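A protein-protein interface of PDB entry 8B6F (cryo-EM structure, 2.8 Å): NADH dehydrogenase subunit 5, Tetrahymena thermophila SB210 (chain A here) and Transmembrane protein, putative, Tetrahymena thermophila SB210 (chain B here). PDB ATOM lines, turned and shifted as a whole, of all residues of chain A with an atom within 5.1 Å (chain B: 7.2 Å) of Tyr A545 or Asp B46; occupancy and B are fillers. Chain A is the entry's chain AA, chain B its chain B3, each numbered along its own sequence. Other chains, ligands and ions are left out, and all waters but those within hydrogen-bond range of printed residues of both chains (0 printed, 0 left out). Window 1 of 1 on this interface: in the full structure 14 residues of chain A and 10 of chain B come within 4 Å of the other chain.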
ATOM      1  N   GLY A 543      -7.130 -17.260  12.885  1.00  0.00           N
ATOM      2  CA  GLY A 543      -7.331 -16.070  13.695  1.00  0.00           C
ATOM      3  C   GLY A 543      -6.832 -16.217  15.115  1.00  0.00           C
ATOM      4  O   GLY A 543      -7.469 -15.714  16.050  1.00  0.00           O
ATOM      5  N   PHE A 544      -5.706 -16.901  15.303  1.00  0.00           N
ATOM      6  CA  PHE A 544      -5.112 -17.075  16.621  1.00  0.00           C
ATOM      7  C   PHE A 544      -4.148 -15.957  16.987  1.00  0.00           C
ATOM      8  O   PHE A 544      -3.592 -15.978  18.088  1.00  0.00           O
ATOM      9  CB  PHE A 544      -4.375 -18.418  16.702  1.00  0.00           C
ATOM     10  CG  PHE A 544      -5.279 -19.612  16.863  1.00  0.00           C
ATOM     11  CD1 PHE A 544      -6.654 -19.501  16.722  1.00  0.00           C
ATOM     12  CD2 PHE A 544      -4.744 -20.852  17.168  1.00  0.00           C
ATOM     13  CE1 PHE A 544      -7.472 -20.603  16.877  1.00  0.00           C
ATOM     14  CE2 PHE A 544      -5.557 -21.956  17.323  1.00  0.00           C
ATOM     15  CZ  PHE A 544      -6.922 -21.832  17.177  1.00  0.00           C
ATOM     16  N   TYR A 545      -3.935 -14.986  16.100  1.00  0.00           N
ATOM     17  CA  TYR A 545      -2.989 -13.918  16.401  1.00  0.00           C
ATOM     18  C   TYR A 545      -3.424 -13.136  17.635  1.00  0.00           C
ATOM     19  O   TYR A 545      -2.593 -12.774  18.474  1.00  0.00           O
ATOM     20  CB  TYR A 545      -2.852 -12.980  15.202  1.00  0.00           C
ATOM     21  CG  TYR A 545      -4.051 -12.086  15.017  1.00  0.00           C
ATOM     22  CD1 TYR A 545      -5.190 -12.544  14.370  1.00  0.00           C
ATOM     23  CD2 TYR A 545      -4.055 -10.793  15.515  1.00  0.00           C
ATOM     24  CE1 TYR A 545      -6.292 -11.734  14.211  1.00  0.00           C
ATOM     25  CE2 TYR A 545      -5.151  -9.975  15.364  1.00  0.00           C
ATOM     26  CZ  TYR A 545      -6.268 -10.454  14.714  1.00  0.00           C
ATOM     27  OH  TYR A 545      -7.360  -9.635  14.559  1.00  0.00           O
ATOM     28  N   LYS A 546      -4.725 -12.860  17.757  1.00  0.00           N
ATOM     29  CA  LYS A 546      -5.219 -12.093  18.891  1.00  0.00           C
ATOM     30  C   LYS A 546      -5.287 -12.929  20.162  1.00  0.00           C
ATOM     31  O   LYS A 546      -5.060 -12.405  21.256  1.00  0.00           O
ATOM     32  CB  LYS A 546      -6.600 -11.518  18.572  1.00  0.00           C
ATOM     33  CG  LYS A 546      -7.032 -10.429  19.534  1.00  0.00           C
ATOM     34  CD  LYS A 546      -8.480 -10.018  19.332  1.00  0.00           C
ATOM     35  CE  LYS A 546      -8.683  -9.300  18.014  1.00  0.00           C
ATOM     36  NZ  LYS A 546     -10.050  -8.721  17.922  1.00  0.00           N
ATOM     37  N   TYR A 547      -5.606 -14.218  20.040  1.00  0.00           N
ATOM     38  CA  TYR A 547      -5.725 -15.073  21.213  1.00  0.00           C
ATOM     39  C   TYR A 547      -4.368 -15.475  21.769  1.00  0.00           C
ATOM     40  O   TYR A 547      -4.255 -15.747  22.970  1.00  0.00           O
ATOM     41  CB  TYR A 547      -6.551 -16.313  20.874  1.00  0.00           C
ATOM     42  CG  TYR A 547      -7.999 -15.995  20.598  1.00  0.00           C
ATOM     43  CD1 TYR A 547      -8.419 -15.615  19.332  1.00  0.00           C
ATOM     44  CD2 TYR A 547      -8.947 -16.065  21.609  1.00  0.00           C
ATOM     45  CE1 TYR A 547      -9.742 -15.318  19.079  1.00  0.00           C
ATOM     46  CE2 TYR A 547     -10.272 -15.771  21.367  1.00  0.00           C
ATOM     47  CZ  TYR A 547     -10.663 -15.397  20.100  1.00  0.00           C
ATOM     48  OH  TYR A 547     -11.982 -15.103  19.856  1.00  0.00           O
ATOM     49  N   LEU A 548      -3.336 -15.513  20.931  1.00  0.00           N
ATOM     50  CA  LEU A 548      -1.974 -15.833  21.356  1.00  0.00           C
ATOM     51  C   LEU A 548      -1.026 -14.789  20.786  1.00  0.00           C
ATOM     52  O   LEU A 548      -0.226 -15.077  19.889  1.00  0.00           O
ATOM     53  CB  LEU A 548      -1.572 -17.237  20.906  1.00  0.00           C
ATOM     54  CG  LEU A 548      -2.512 -18.377  21.300  1.00  0.00           C
ATOM     55  CD1 LEU A 548      -2.151 -19.635  20.542  1.00  0.00           C
ATOM     56  CD2 LEU A 548      -2.446 -18.625  22.791  1.00  0.00           C
ATOM     57  N   PRO A 549      -1.093 -13.552  21.284  1.00  0.00           N
ATOM     58  CA  PRO A 549      -0.242 -12.498  20.706  1.00  0.00           C
ATOM     59  C   PRO A 549       1.240 -12.813  20.779  1.00  0.00           C
ATOM     60  O   PRO A 549       1.955 -12.660  19.782  1.00  0.00           O
ATOM     61  CB  PRO A 549      -0.609 -11.260  21.539  1.00  0.00           C
ATOM     62  CG  PRO A 549      -1.920 -11.577  22.155  1.00  0.00           C
ATOM     63  CD  PRO A 549      -1.922 -13.045  22.388  1.00  0.00           C
ATOM     64  N   CYS A 552       2.364 -15.535  18.276  1.00  0.00           N
ATOM     65  CA  CYS A 552       2.424 -15.097  16.886  1.00  0.00           C
ATOM     66  C   CYS A 552       3.768 -14.454  16.576  1.00  0.00           C
ATOM     67  O   CYS A 552       4.447 -14.837  15.617  1.00  0.00           O
ATOM     68  CB  CYS A 552       1.283 -14.122  16.599  1.00  0.00           C
ATOM     69  SG  CYS A 552       1.312 -13.426  14.937  1.00  0.00           S
ATOM     70  N   PHE A 614      -2.192 -18.423  12.422  1.00  0.00           N
ATOM     71  CA  PHE A 614      -2.487 -17.144  13.055  1.00  0.00           C
ATOM     72  C   PHE A 614      -3.437 -16.265  12.252  1.00  0.00           C
ATOM     73  O   PHE A 614      -4.485 -15.869  12.769  1.00  0.00           O
ATOM     74  CB  PHE A 614      -1.168 -16.405  13.323  1.00  0.00           C
ATOM     75  CG  PHE A 614      -0.262 -17.126  14.280  1.00  0.00           C
ATOM     76  CD1 PHE A 614      -0.530 -17.124  15.638  1.00  0.00           C
ATOM     77  CD2 PHE A 614       0.847 -17.817  13.822  1.00  0.00           C
ATOM     78  CE1 PHE A 614       0.294 -17.790  16.522  1.00  0.00           C
ATOM     79  CE2 PHE A 614       1.674 -18.487  14.701  1.00  0.00           C
ATOM     80  CZ  PHE A 614       1.396 -18.473  16.054  1.00  0.00           C
ATOM     81  N   PHE A 615      -3.112 -15.945  11.000  1.00  0.00           N
ATOM     82  CA  PHE A 615      -3.802 -14.877  10.287  1.00  0.00           C
ATOM     83  C   PHE A 615      -4.781 -15.374   9.231  1.00  0.00           C
ATOM     84  O   PHE A 615      -5.317 -14.563   8.471  1.00  0.00           O
ATOM     85  CB  PHE A 615      -2.782 -13.937   9.643  1.00  0.00           C
ATOM     86  CG  PHE A 615      -2.037 -13.096  10.632  1.00  0.00           C
ATOM     87  CD1 PHE A 615      -2.659 -12.031  11.256  1.00  0.00           C
ATOM     88  CD2 PHE A 615      -0.717 -13.372  10.940  1.00  0.00           C
ATOM     89  CE1 PHE A 615      -1.983 -11.256  12.169  1.00  0.00           C
ATOM     90  CE2 PHE A 615      -0.033 -12.601  11.853  1.00  0.00           C
ATOM     91  CZ  PHE A 615      -0.667 -11.540  12.469  1.00  0.00           C
ATOM     92  N   LYS A 618     -10.942 -17.800  10.474  1.00  0.00           N
ATOM     93  CA  LYS A 618     -11.209 -18.650  11.631  1.00  0.00           C
ATOM     94  C   LYS A 618     -11.833 -19.961  11.167  1.00  0.00           C
ATOM     95  O   LYS A 618     -12.987 -19.989  10.727  1.00  0.00           O
ATOM     96  CB  LYS A 618     -12.117 -17.925  12.620  1.00  0.00           C
ATOM     97  CG  LYS A 618     -11.453 -16.724  13.279  1.00  0.00           C
ATOM     98  CD  LYS A 618     -12.252 -16.203  14.463  1.00  0.00           C
ATOM     99  CE  LYS A 618     -13.579 -15.613  14.026  1.00  0.00           C
ATOM    100  NZ  LYS A 618     -14.332 -15.031  15.174  1.00  0.00           N
ATOM    101  N   TYR A 625     -13.006 -20.248  20.359  1.00  0.00           N
ATOM    102  CA  TYR A 625     -12.990 -18.791  20.406  1.00  0.00           C
ATOM    103  C   TYR A 625     -13.940 -18.242  21.464  1.00  0.00           C
ATOM    104  O   TYR A 625     -13.589 -17.303  22.185  1.00  0.00           O
ATOM    105  CB  TYR A 625     -13.349 -18.227  19.034  1.00  0.00           C
ATOM    106  CG  TYR A 625     -12.503 -18.777  17.914  1.00  0.00           C
ATOM    107  CD1 TYR A 625     -11.250 -18.246  17.646  1.00  0.00           C
ATOM    108  CD2 TYR A 625     -12.955 -19.824  17.124  1.00  0.00           C
ATOM    109  CE1 TYR A 625     -10.470 -18.738  16.627  1.00  0.00           C
ATOM    110  CE2 TYR A 625     -12.180 -20.326  16.098  1.00  0.00           C
ATOM    111  CZ  TYR A 625     -10.938 -19.777  15.856  1.00  0.00           C
ATOM    112  OH  TYR A 625     -10.156 -20.263  14.840  1.00  0.00           O
ATOM    113  N   TRP B  40     -20.607 -16.140  12.385  1.00  0.00           N
ATOM    114  CA  TRP B  40     -19.642 -15.717  13.393  1.00  0.00           C
ATOM    115  C   TRP B  40     -18.204 -15.797  12.897  1.00  0.00           C
ATOM    116  O   TRP B  40     -17.343 -15.077  13.413  1.00  0.00           O
ATOM    117  CB  TRP B  40     -19.795 -16.573  14.651  1.00  0.00           C
ATOM    118  CG  TRP B  40     -19.369 -17.988  14.463  1.00  0.00           C
ATOM    119  CD1 TRP B  40     -20.151 -19.034  14.078  1.00  0.00           C
ATOM    120  CD2 TRP B  40     -18.052 -18.516  14.651  1.00  0.00           C
ATOM    121  NE1 TRP B  40     -19.403 -20.183  14.014  1.00  0.00           N
ATOM    122  CE2 TRP B  40     -18.110 -19.892  14.360  1.00  0.00           C
ATOM    123  CE3 TRP B  40     -16.829 -17.957  15.033  1.00  0.00           C
ATOM    124  CZ2 TRP B  40     -16.993 -20.718  14.443  1.00  0.00           C
ATOM    125  CZ3 TRP B  40     -15.721 -18.777  15.116  1.00  0.00           C
ATOM    126  CH2 TRP B  40     -15.809 -20.143  14.821  1.00  0.00           C
ATOM    127  N   ARG B  41     -17.924 -16.650  11.909  1.00  0.00           N
ATOM    128  CA  ARG B  41     -16.540 -16.895  11.516  1.00  0.00           C
ATOM    129  C   ARG B  41     -15.874 -15.637  10.977  1.00  0.00           C
ATOM    130  O   ARG B  41     -14.708 -15.365  11.281  1.00  0.00           O
ATOM    131  CB  ARG B  41     -16.482 -18.013  10.477  1.00  0.00           C
ATOM    132  CG  ARG B  41     -16.862 -19.371  11.025  1.00  0.00           C
ATOM    133  CD  ARG B  41     -16.621 -20.466  10.006  1.00  0.00           C
ATOM    134  NE  ARG B  41     -16.854 -21.784  10.583  1.00  0.00           N
ATOM    135  CZ  ARG B  41     -15.982 -22.432  11.343  1.00  0.00           C
ATOM    136  NH1 ARG B  41     -14.809 -21.907  11.649  1.00  0.00           N
ATOM    137  NH2 ARG B  41     -16.300 -23.632  11.816  1.00  0.00           N
ATOM    138  N   TRP B  42     -16.594 -14.855  10.173  1.00  0.00           N
ATOM    139  CA  TRP B  42     -16.011 -13.728   9.457  1.00  0.00           C
ATOM    140  C   TRP B  42     -16.244 -12.401  10.169  1.00  0.00           C
ATOM    141  O   TRP B  42     -16.383 -11.362   9.516  1.00  0.00           O
ATOM    142  CB  TRP B  42     -16.562 -13.677   8.034  1.00  0.00           C
ATOM    143  CG  TRP B  42     -16.724 -15.037   7.443  1.00  0.00           C
ATOM    144  CD1 TRP B  42     -15.731 -15.868   7.005  1.00  0.00           C
ATOM    145  CD2 TRP B  42     -17.953 -15.734   7.234  1.00  0.00           C
ATOM    146  NE1 TRP B  42     -16.272 -17.039   6.532  1.00  0.00           N
ATOM    147  CE2 TRP B  42     -17.634 -16.981   6.662  1.00  0.00           C
ATOM    148  CE3 TRP B  42     -19.293 -15.424   7.473  1.00  0.00           C
ATOM    149  CZ2 TRP B  42     -18.608 -17.915   6.326  1.00  0.00           C
ATOM    150  CZ3 TRP B  42     -20.258 -16.351   7.138  1.00  0.00           C
ATOM    151  CH2 TRP B  42     -19.912 -17.583   6.571  1.00  0.00           C
ATOM    152  N   ASN B  43     -16.288 -12.413  11.498  1.00  0.00           N
ATOM    153  CA  ASN B  43     -16.429 -11.175  12.248  1.00  0.00           C
ATOM    154  C   ASN B  43     -15.217 -10.285  12.010  1.00  0.00           C
ATOM    155  O   ASN B  43     -14.072 -10.722  12.154  1.00  0.00           O
ATOM    156  CB  ASN B  43     -16.582 -11.484  13.738  1.00  0.00           C
ATOM    157  CG  ASN B  43     -16.918 -10.257  14.559  1.00  0.00           C
ATOM    158  OD1 ASN B  43     -16.657  -9.128  14.150  1.00  0.00           O
ATOM    159  ND2 ASN B  43     -17.499 -10.475  15.732  1.00  0.00           N
ATOM    160  N   THR B  44     -15.472  -9.028  11.646  1.00  0.00           N
ATOM    161  CA  THR B  44     -14.382  -8.090  11.409  1.00  0.00           C
ATOM    162  C   THR B  44     -13.755  -7.604  12.708  1.00  0.00           C
ATOM    163  O   THR B  44     -12.579  -7.227  12.718  1.00  0.00           O
ATOM    164  CB  THR B  44     -14.879  -6.900  10.588  1.00  0.00           C
ATOM    165  OG1 THR B  44     -16.084  -6.384  11.167  1.00  0.00           O
ATOM    166  CG2 THR B  44     -15.143  -7.320   9.152  1.00  0.00           C
ATOM    167  N   LYS B  45     -14.515  -7.603  13.803  1.00  0.00           N
ATOM    168  CA  LYS B  45     -13.982  -7.205  15.100  1.00  0.00           C
ATOM    169  C   LYS B  45     -12.972  -8.198  15.658  1.00  0.00           C
ATOM    170  O   LYS B  45     -12.280  -7.868  16.625  1.00  0.00           O
ATOM    171  CB  LYS B  45     -15.122  -7.033  16.106  1.00  0.00           C
ATOM    172  CG  LYS B  45     -15.868  -5.717  15.986  1.00  0.00           C
ATOM    173  CD  LYS B  45     -17.049  -5.638  16.941  1.00  0.00           C
ATOM    174  CE  LYS B  45     -18.165  -6.589  16.539  1.00  0.00           C
ATOM    175  NZ  LYS B  45     -19.358  -6.445  17.418  1.00  0.00           N
ATOM    176  N   ASP B  46     -12.869  -9.395  15.080  1.00  0.00           N
ATOM    177  CA  ASP B  46     -12.073 -10.465  15.659  1.00  0.00           C
ATOM    178  C   ASP B  46     -10.871 -10.873  14.818  1.00  0.00           C
ATOM    179  O   ASP B  46     -10.015 -11.608  15.320  1.00  0.00           O
ATOM    180  CB  ASP B  46     -12.956 -11.699  15.897  1.00  0.00           C
ATOM    181  CG  ASP B  46     -12.328 -12.693  16.856  1.00  0.00           C
ATOM    182  OD1 ASP B  46     -11.309 -12.350  17.488  1.00  0.00           O
ATOM    183  OD2 ASP B  46     -12.856 -13.818  16.977  1.00  0.00           O
ATOM    184  N   ASN B  47     -10.780 -10.436  13.563  1.00  0.00           N
ATOM    185  CA  ASN B  47      -9.692 -10.850  12.687  1.00  0.00           C
ATOM    186  C   ASN B  47      -9.136  -9.646  11.938  1.00  0.00           C
ATOM    187  O   ASN B  47      -9.861  -8.694  11.638  1.00  0.00           O
ATOM    188  CB  ASN B  47     -10.157 -11.921  11.694  1.00  0.00           C
ATOM    189  CG  ASN B  47      -9.001 -12.677  11.077  1.00  0.00           C
ATOM    190  OD1 ASN B  47      -7.912 -12.134  10.904  1.00  0.00           O
ATOM    191  ND2 ASN B  47      -9.229 -13.943  10.751  1.00  0.00           N
ATOM    192  N   THR B  48      -7.840  -9.702  11.636  1.00  0.00           N
ATOM    193  CA  THR B  48      -7.156  -8.649  10.893  1.00  0.00           C
ATOM    194  C   THR B  48      -6.139  -9.314   9.971  1.00  0.00           C
ATOM    195  O   THR B  48      -6.160 -10.531   9.767  1.00  0.00           O
ATOM    196  CB  THR B  48      -6.505  -7.632  11.844  1.00  0.00           C
ATOM    197  OG1 THR B  48      -6.210  -6.428  11.127  1.00  0.00           O
ATOM    198  CG2 THR B  48      -5.195  -8.162  12.417  1.00  0.00           C
ATOM    199  N   THR B  49      -5.240  -8.512   9.411  1.00  0.00           N
ATOM    200  CA  THR B  49      -4.216  -8.987   8.496  1.00  0.00           C
ATOM    201  C   THR B  49      -2.843  -8.883   9.148  1.00  0.00           C
ATOM    202  O   THR B  49      -2.621  -8.088  10.064  1.00  0.00           O
ATOM    203  CB  THR B  49      -4.230  -8.190   7.187  1.00  0.00           C
ATOM    204  OG1 THR B  49      -3.704  -6.877   7.414  1.00  0.00           O
ATOM    205  CG2 THR B  49      -5.644  -8.071   6.651  1.00  0.00           C
ATOM    206  N   ALA B  50      -1.917  -9.701   8.654  1.00  0.00           N
ATOM    207  CA  ALA B  50      -0.566  -9.708   9.208  1.00  0.00           C
ATOM    208  C   ALA B  50       0.123  -8.355   9.104  1.00  0.00           C
ATOM    209  O   ALA B  50       0.751  -7.938  10.093  1.00  0.00           O
ATOM    210  CB  ALA B  50       0.267 -10.798   8.522  1.00  0.00           C
ATOM    211  N   PHE B  53      -1.243  -6.257  11.948  1.00  0.00           N
ATOM    212  CA  PHE B  53      -0.851  -6.671  13.292  1.00  0.00           C
ATOM    213  C   PHE B  53       0.622  -6.386  13.558  1.00  0.00           C
ATOM    214  O   PHE B  53       0.985  -5.951  14.657  1.00  0.00           O
ATOM    215  CB  PHE B  53      -1.148  -8.156  13.495  1.00  0.00           C
ATOM    216  CG  PHE B  53      -0.862  -8.642  14.888  1.00  0.00           C
ATOM    217  CD1 PHE B  53      -1.691  -8.293  15.941  1.00  0.00           C
ATOM    218  CD2 PHE B  53       0.232  -9.451  15.143  1.00  0.00           C
ATOM    219  CE1 PHE B  53      -1.433  -8.740  17.221  1.00  0.00           C
ATOM    220  CE2 PHE B  53       0.497  -9.901  16.421  1.00  0.00           C
ATOM    221  CZ  PHE B  53      -0.337  -9.546  17.461  1.00  0.00           C
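OH of Tyr A545 sits at hydrogen-bond distance from O of Asp B46.
The side-chain hydroxyl of Tyr A545 sits at hydrogen-bond distance from the backbone NH of Thr B48.
The backbone carbonyl oxygen (O) of Lys B45 lies within hydrogen-bond range of the side-chain amino group (NZ) of Lys A546, at 2.7 Å.
The side-chain amino group (NZ) of Lys A546 is in salt-bridge range of the side-chain carboxylate (OD1) of Asp B46, at 3.9 Å.
The side-chain carboxylate (OD2) of Asp B46 lies within hydrogen-bond range of the side-chain hydroxyl (OH) of Tyr A547 (3.3 Å).
O of Trp B40 sits at hydrogen-bond distance from NZ of Lys A618 (3.5 Å).
The guanidinium group of Arg B41 is in hydrogen-bond range of the backbone carbonyl oxygen of Lys A618 (2.8 Å).
The side-chain amino group (NZ) of Lys A618 is in salt-bridge range of the side-chain carboxylate (OD2) of Asp B46, 2.6 Å away.
N of Tyr A545 lies within hydrogen-bond range of O of Phe A614 (3.5 Å).
The backbone NH of Lys B45 is in hydrogen-bond range of the side-chain amide oxygen of Asn B43 (2.7 Å).
Among the printed residues, merely in contact across the chains: Tyr A545 with Asn B47 (3.2 Å), Tyr A545 with Phe B53 (3.5 Å), Phe A615 with Phe B53 (3.5 Å), Phe A615 with Ala B50 (3.6 Å), Tyr A625 with Trp B40 (3.6 Å), Phe A615 with Thr B49 (3.8 Å) and Cys A552 with Phe B53 (3.9 Å).
Of chain B, only Asp B46, Asn B47, Thr B48 and Phe B53 come within 4 Å of Tyr A545.
Asp B46 touches four residues of chain A.
Of the printed residues of chain B, Tyr A547 touches Asp B46 (3.3 Å).
Of the printed residues of chain B, Cys A552 touches Phe B53.
Printed residues of chain A within 4 Å of Thr B48: Tyr A545.
Printed residues of chain B within 4 Å of Phe A615: Thr B49, Ala B50 and Phe B53.
Of the printed residues of chain A, Thr B49 touches Phe A615.
Asn B43 touches none of the printed residues of chain A.
Phe A544 touches none of the printed residues of chain B.
Hydrophobic or aromatic side chains of chain A within 4 Å of the printed part of chain B: Tyr A545, Tyr A547, Phe A615 and Tyr A625.
Along chain A the printed residues that touch a printed residue of chain B span positions 545 to 625.
Hydrophobic or aromatic side chains of chain B within 4 Å of the printed part of chain A: Trp B40, Ala B50 and Phe B53.
Among the printed residues, 15 pairs touch across the chains.
Among the printed residues, Asp or Glu carboxylates within 4 Å of a Lys or Arg side-chain nitrogen of the other chain: Lys A546 with Asp B46 and Lys A618 with Asp B46.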
